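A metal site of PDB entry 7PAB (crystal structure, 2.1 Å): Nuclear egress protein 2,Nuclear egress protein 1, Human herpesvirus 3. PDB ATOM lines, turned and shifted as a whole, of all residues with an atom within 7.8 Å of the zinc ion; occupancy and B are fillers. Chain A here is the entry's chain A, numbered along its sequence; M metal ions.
The zinc ion is bound by NE2 of His 364 (2.1 Å), SG of Cys 260 (2.3 Å), SG of Cys 241 (2.3 Å) and SG of Cys 257 (2.3 Å).
O of Cys 260 sits at hydrogen-bond distance from NE2 of His 366 (3.4 Å).
O of Cys 241 lies within hydrogen-bond range of N of Gly 252 (2.9 Å).
The side-chain sulfur of Cys 257 sits close to the backbone NH of Thr 259 (3.6 Å).
O of Cys 257 is in hydrogen-bond range of OG1 of Thr 261 (3.0 Å).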
ATOM      1  N   ASP A 239     -18.912  -7.548 -29.344  1.00  0.00           N
ATOM      2  CA  ASP A 239     -19.060  -7.646 -27.896  1.00  0.00           C
ATOM      3  C   ASP A 239     -19.411  -6.305 -27.253  1.00  0.00           C
ATOM      4  O   ASP A 239     -19.391  -6.199 -26.024  1.00  0.00           O
ATOM      5  CB  ASP A 239     -17.784  -8.208 -27.263  1.00  0.00           C
ATOM      6  CG  ASP A 239     -16.623  -7.240 -27.322  1.00  0.00           C
ATOM      7  OD1 ASP A 239     -16.634  -6.347 -28.189  1.00  0.00           O
ATOM      8  OD2 ASP A 239     -15.702  -7.379 -26.492  1.00  0.00           O
ATOM      9  N   ASN A 240     -19.744  -5.295 -28.055  1.00  0.00           N
ATOM     10  CA  ASN A 240     -20.159  -4.009 -27.509  1.00  0.00           C
ATOM     11  C   ASN A 240     -21.629  -4.048 -27.094  1.00  0.00           C
ATOM     12  O   ASN A 240     -22.483  -4.483 -27.865  1.00  0.00           O
ATOM     13  CB  ASN A 240     -19.967  -2.889 -28.527  1.00  0.00           C
ATOM     14  CG  ASN A 240     -18.535  -2.381 -28.603  1.00  0.00           C
ATOM     15  OD1 ASN A 240     -18.012  -2.167 -29.688  1.00  0.00           O
ATOM     16  ND2 ASN A 240     -17.914  -2.184 -27.450  1.00  0.00           N
ATOM     17  N   CYS A 241     -21.901  -3.580 -25.886  1.00  0.00           N
ATOM     18  CA  CYS A 241     -23.254  -3.239 -25.467  1.00  0.00           C
ATOM     19  C   CYS A 241     -23.390  -1.718 -25.436  1.00  0.00           C
ATOM     20  O   CYS A 241     -22.396  -0.991 -25.451  1.00  0.00           O
ATOM     21  CB  CYS A 241     -23.577  -3.843 -24.093  1.00  0.00           C
ATOM     22  SG  CYS A 241     -22.585  -3.193 -22.719  1.00  0.00           S
ATOM     23  N   LEU A 242     -24.631  -1.248 -25.402  1.00  0.00           N
ATOM     24  CA  LEU A 242     -24.921   0.176 -25.425  1.00  0.00           C
ATOM     25  C   LEU A 242     -25.848   0.530 -24.275  1.00  0.00           C
ATOM     26  O   LEU A 242     -26.903  -0.080 -24.107  1.00  0.00           O
ATOM     27  CB  LEU A 242     -25.547   0.591 -26.755  1.00  0.00           C
ATOM     28  CG  LEU A 242     -25.775   2.094 -26.933  1.00  0.00           C
ATOM     29  CD1 LEU A 242     -24.447   2.847 -26.985  1.00  0.00           C
ATOM     30  CD2 LEU A 242     -26.576   2.365 -28.198  1.00  0.00           C
ATOM     31  N   SER A 243     -25.453   1.522 -23.478  1.00  0.00           N
ATOM     32  CA  SER A 243     -26.205   1.980 -22.329  1.00  0.00           C
ATOM     33  C   SER A 243     -26.569   3.443 -22.516  1.00  0.00           C
ATOM     34  O   SER A 243     -25.678   4.279 -22.752  1.00  0.00           O
ATOM     35  CB  SER A 243     -25.406   1.791 -21.038  1.00  0.00           C
ATOM     36  OG  SER A 243     -26.084   2.374 -19.926  1.00  0.00           O
ATOM     37  N   HIS A 250     -22.893   5.388 -23.196  1.00  0.00           N
ATOM     38  CA  HIS A 250     -21.653   4.642 -23.068  1.00  0.00           C
ATOM     39  C   HIS A 250     -21.718   3.317 -23.811  1.00  0.00           C
ATOM     40  O   HIS A 250     -22.763   2.660 -23.822  1.00  0.00           O
ATOM     41  CB  HIS A 250     -21.325   4.394 -21.587  1.00  0.00           C
ATOM     42  CG  HIS A 250     -21.414   5.609 -20.723  1.00  0.00           C
ATOM     43  ND1 HIS A 250     -20.486   6.634 -20.790  1.00  0.00           N
ATOM     44  CD2 HIS A 250     -22.315   5.976 -19.791  1.00  0.00           C
ATOM     45  CE1 HIS A 250     -20.822   7.573 -19.927  1.00  0.00           C
ATOM     46  NE2 HIS A 250     -21.928   7.209 -19.305  1.00  0.00           N
ATOM     47  N   LEU A 251     -20.600   2.950 -24.440  1.00  0.00           N
ATOM     48  CA  LEU A 251     -20.397   1.595 -24.919  1.00  0.00           C
ATOM     49  C   LEU A 251     -19.680   0.781 -23.852  1.00  0.00           C
ATOM     50  O   LEU A 251     -18.776   1.287 -23.178  1.00  0.00           O
ATOM     51  CB  LEU A 251     -19.563   1.578 -26.203  1.00  0.00           C
ATOM     52  CG  LEU A 251     -20.264   1.806 -27.533  1.00  0.00           C
ATOM     53  CD1 LEU A 251     -19.229   1.733 -28.654  1.00  0.00           C
ATOM     54  CD2 LEU A 251     -21.377   0.790 -27.760  1.00  0.00           C
ATOM     55  N   GLY A 252     -20.097  -0.479 -23.692  1.00  0.00           N
ATOM     56  CA  GLY A 252     -19.501  -1.370 -22.730  1.00  0.00           C
ATOM     57  C   GLY A 252     -18.896  -2.592 -23.401  1.00  0.00           C
ATOM     58  O   GLY A 252     -19.108  -2.853 -24.584  1.00  0.00           O
ATOM     59  N   LEU A 253     -18.118  -3.339 -22.616  1.00  0.00           N
ATOM     60  CA  LEU A 253     -17.567  -4.608 -23.044  1.00  0.00           C
ATOM     61  C   LEU A 253     -18.465  -5.719 -22.506  1.00  0.00           C
ATOM     62  O   LEU A 253     -18.609  -5.865 -21.282  1.00  0.00           O
ATOM     63  CB  LEU A 253     -16.130  -4.780 -22.558  1.00  0.00           C
ATOM     64  CG  LEU A 253     -15.142  -3.710 -23.039  1.00  0.00           C
ATOM     65  CD1 LEU A 253     -13.743  -4.011 -22.557  1.00  0.00           C
ATOM     66  CD2 LEU A 253     -15.172  -3.595 -24.556  1.00  0.00           C
ATOM     67  N   GLY A 254     -19.074  -6.483 -23.410  1.00  0.00           N
ATOM     68  CA  GLY A 254     -20.058  -7.463 -23.006  1.00  0.00           C
ATOM     69  C   GLY A 254     -19.583  -8.376 -21.901  1.00  0.00           C
ATOM     70  O   GLY A 254     -20.333  -8.695 -20.974  1.00  0.00           O
ATOM     71  N   GLY A 255     -18.323  -8.809 -21.965  1.00  0.00           N
ATOM     72  CA  GLY A 255     -17.810  -9.722 -20.967  1.00  0.00           C
ATOM     73  C   GLY A 255     -17.656  -9.087 -19.597  1.00  0.00           C
ATOM     74  O   GLY A 255     -17.754  -9.778 -18.573  1.00  0.00           O
ATOM     75  N   TYR A 256     -17.423  -7.779 -19.546  1.00  0.00           N
ATOM     76  CA  TYR A 256     -17.144  -7.072 -18.301  1.00  0.00           C
ATOM     77  C   TYR A 256     -18.262  -6.119 -17.913  1.00  0.00           C
ATOM     78  O   TYR A 256     -18.098  -5.333 -16.963  1.00  0.00           O
ATOM     79  CB  TYR A 256     -15.817  -6.329 -18.418  1.00  0.00           C
ATOM     80  CG  TYR A 256     -14.712  -7.179 -19.011  1.00  0.00           C
ATOM     81  CD1 TYR A 256     -14.582  -7.329 -20.381  1.00  0.00           C
ATOM     82  CD2 TYR A 256     -13.806  -7.840 -18.195  1.00  0.00           C
ATOM     83  CE1 TYR A 256     -13.579  -8.123 -20.925  1.00  0.00           C
ATOM     84  CE2 TYR A 256     -12.794  -8.629 -18.729  1.00  0.00           C
ATOM     85  CZ  TYR A 256     -12.693  -8.756 -20.096  1.00  0.00           C
ATOM     86  OH  TYR A 256     -11.691  -9.543 -20.634  1.00  0.00           O
ATOM     87  N   CYS A 257     -19.399  -6.154 -18.611  1.00  0.00           N
ATOM     88  CA  CYS A 257     -20.551  -5.340 -18.246  1.00  0.00           C
ATOM     89  C   CYS A 257     -21.405  -6.111 -17.250  1.00  0.00           C
ATOM     90  O   CYS A 257     -21.857  -7.226 -17.569  1.00  0.00           O
ATOM     91  CB  CYS A 257     -21.367  -4.983 -19.474  1.00  0.00           C
ATOM     92  SG  CYS A 257     -22.951  -4.160 -19.139  1.00  0.00           S
ATOM     93  N   PRO A 258     -21.645  -5.593 -16.038  1.00  0.00           N
ATOM     94  CA  PRO A 258     -22.494  -6.331 -15.097  1.00  0.00           C
ATOM     95  C   PRO A 258     -23.876  -6.627 -15.639  1.00  0.00           C
ATOM     96  O   PRO A 258     -24.389  -7.746 -15.454  1.00  0.00           O
ATOM     97  CB  PRO A 258     -22.542  -5.414 -13.866  1.00  0.00           C
ATOM     98  CG  PRO A 258     -21.332  -4.555 -13.977  1.00  0.00           C
ATOM     99  CD  PRO A 258     -21.108  -4.354 -15.452  1.00  0.00           C
ATOM    100  N   THR A 259     -24.508  -5.661 -16.300  1.00  0.00           N
ATOM    101  CA  THR A 259     -25.859  -5.883 -16.820  1.00  0.00           C
ATOM    102  C   THR A 259     -25.879  -7.014 -17.843  1.00  0.00           C
ATOM    103  O   THR A 259     -26.698  -7.940 -17.745  1.00  0.00           O
ATOM    104  CB  THR A 259     -26.397  -4.589 -17.447  1.00  0.00           C
ATOM    105  OG1 THR A 259     -26.206  -3.498 -16.535  1.00  0.00           O
ATOM    106  CG2 THR A 259     -27.877  -4.734 -17.771  1.00  0.00           C
ATOM    107  N   CYS A 260     -24.977  -6.967 -18.820  1.00  0.00           N
ATOM    108  CA  CYS A 260     -24.933  -8.004 -19.842  1.00  0.00           C
ATOM    109  C   CYS A 260     -24.730  -9.378 -19.209  1.00  0.00           C
ATOM    110  O   CYS A 260     -25.546 -10.296 -19.388  1.00  0.00           O
ATOM    111  CB  CYS A 260     -23.814  -7.713 -20.847  1.00  0.00           C
ATOM    112  SG  CYS A 260     -24.245  -6.505 -22.103  1.00  0.00           S
ATOM    113  N   THR A 261     -23.637  -9.547 -18.454  1.00  0.00           N
ATOM    114  CA  THR A 261     -23.338 -10.844 -17.860  1.00  0.00           C
ATOM    115  C   THR A 261     -24.494 -11.375 -17.023  1.00  0.00           C
ATOM    116  O   THR A 261     -24.687 -12.591 -16.945  1.00  0.00           O
ATOM    117  CB  THR A 261     -22.068 -10.746 -17.006  1.00  0.00           C
ATOM    118  OG1 THR A 261     -22.241  -9.729 -16.002  1.00  0.00           O
ATOM    119  CG2 THR A 261     -20.861 -10.411 -17.868  1.00  0.00           C
ATOM    120  N   HIS A 364     -30.597  -0.533 -21.917  1.00  0.00           N
ATOM    121  CA  HIS A 364     -29.359  -1.265 -22.106  1.00  0.00           C
ATOM    122  C   HIS A 364     -29.600  -2.295 -23.207  1.00  0.00           C
ATOM    123  O   HIS A 364     -30.488  -3.137 -23.075  1.00  0.00           O
ATOM    124  CB  HIS A 364     -28.896  -1.949 -20.825  1.00  0.00           C
ATOM    125  CG  HIS A 364     -27.751  -2.906 -21.016  1.00  0.00           C
ATOM    126  ND1 HIS A 364     -27.937  -4.258 -21.136  1.00  0.00           N
ATOM    127  CD2 HIS A 364     -26.420  -2.695 -21.117  1.00  0.00           C
ATOM    128  CE1 HIS A 364     -26.764  -4.849 -21.298  1.00  0.00           C
ATOM    129  NE2 HIS A 364     -25.832  -3.916 -21.284  1.00  0.00           N
ATOM    130  N   LEU A 365     -28.820  -2.209 -24.275  1.00  0.00           N
ATOM    131  CA  LEU A 365     -28.916  -3.143 -25.386  1.00  0.00           C
ATOM    132  C   LEU A 365     -27.792  -4.160 -25.254  1.00  0.00           C
ATOM    133  O   LEU A 365     -26.616  -3.830 -25.481  1.00  0.00           O
ATOM    134  CB  LEU A 365     -28.847  -2.403 -26.725  1.00  0.00           C
ATOM    135  CG  LEU A 365     -29.936  -1.349 -26.963  1.00  0.00           C
ATOM    136  CD1 LEU A 365     -29.766  -0.685 -28.327  1.00  0.00           C
ATOM    137  CD2 LEU A 365     -31.319  -1.962 -26.850  1.00  0.00           C
ATOM    138  N   HIS A 366     -28.144  -5.390 -24.889  1.00  0.00           N
ATOM    139  CA  HIS A 366     -27.163  -6.466 -24.759  1.00  0.00           C
ATOM    140  C   HIS A 366     -26.365  -6.599 -26.047  1.00  0.00           C
ATOM    141  O   HIS A 366     -26.890  -6.431 -27.147  1.00  0.00           O
ATOM    142  CB  HIS A 366     -27.891  -7.781 -24.431  1.00  0.00           C
ATOM    143  CG  HIS A 366     -27.006  -8.859 -23.912  1.00  0.00           C
ATOM    144  ND1 HIS A 366     -26.279  -9.688 -24.737  1.00  0.00           N
ATOM    145  CD2 HIS A 366     -26.732  -9.265 -22.654  1.00  0.00           C
ATOM    146  CE1 HIS A 366     -25.592 -10.548 -24.012  1.00  0.00           C
ATOM    147  NE2 HIS A 366     -25.852 -10.313 -22.740  1.00  0.00           N
ATOM    148  N   TYR A 367     -25.075  -6.912 -25.906  1.00  0.00           N
ATOM    149  CA  TYR A 367     -24.211  -6.997 -27.074  1.00  0.00           C
ATOM    150  C   TYR A 367     -24.740  -8.032 -28.066  1.00  0.00           C
ATOM    151  O   TYR A 367     -24.650  -7.837 -29.291  1.00  0.00           O
ATOM    152  CB  TYR A 367     -22.779  -7.324 -26.667  1.00  0.00           C
ATOM    153  CG  TYR A 367     -22.568  -8.702 -26.091  1.00  0.00           C
ATOM    154  CD1 TYR A 367     -22.322  -9.793 -26.920  1.00  0.00           C
ATOM    155  CD2 TYR A 367     -22.595  -8.920 -24.723  1.00  0.00           C
ATOM    156  CE1 TYR A 367     -22.121 -11.062 -26.399  1.00  0.00           C
ATOM    157  CE2 TYR A 367     -22.394 -10.181 -24.195  1.00  0.00           C
ATOM    158  CZ  TYR A 367     -22.160 -11.240 -25.032  1.00  0.00           C
ATOM    159  OH  TYR A 367     -21.960 -12.502 -24.504  1.00  0.00           O
HETATM  160 ZN    ZN M   1     -23.827  -4.438 -21.272  1.00  0.00          ZN
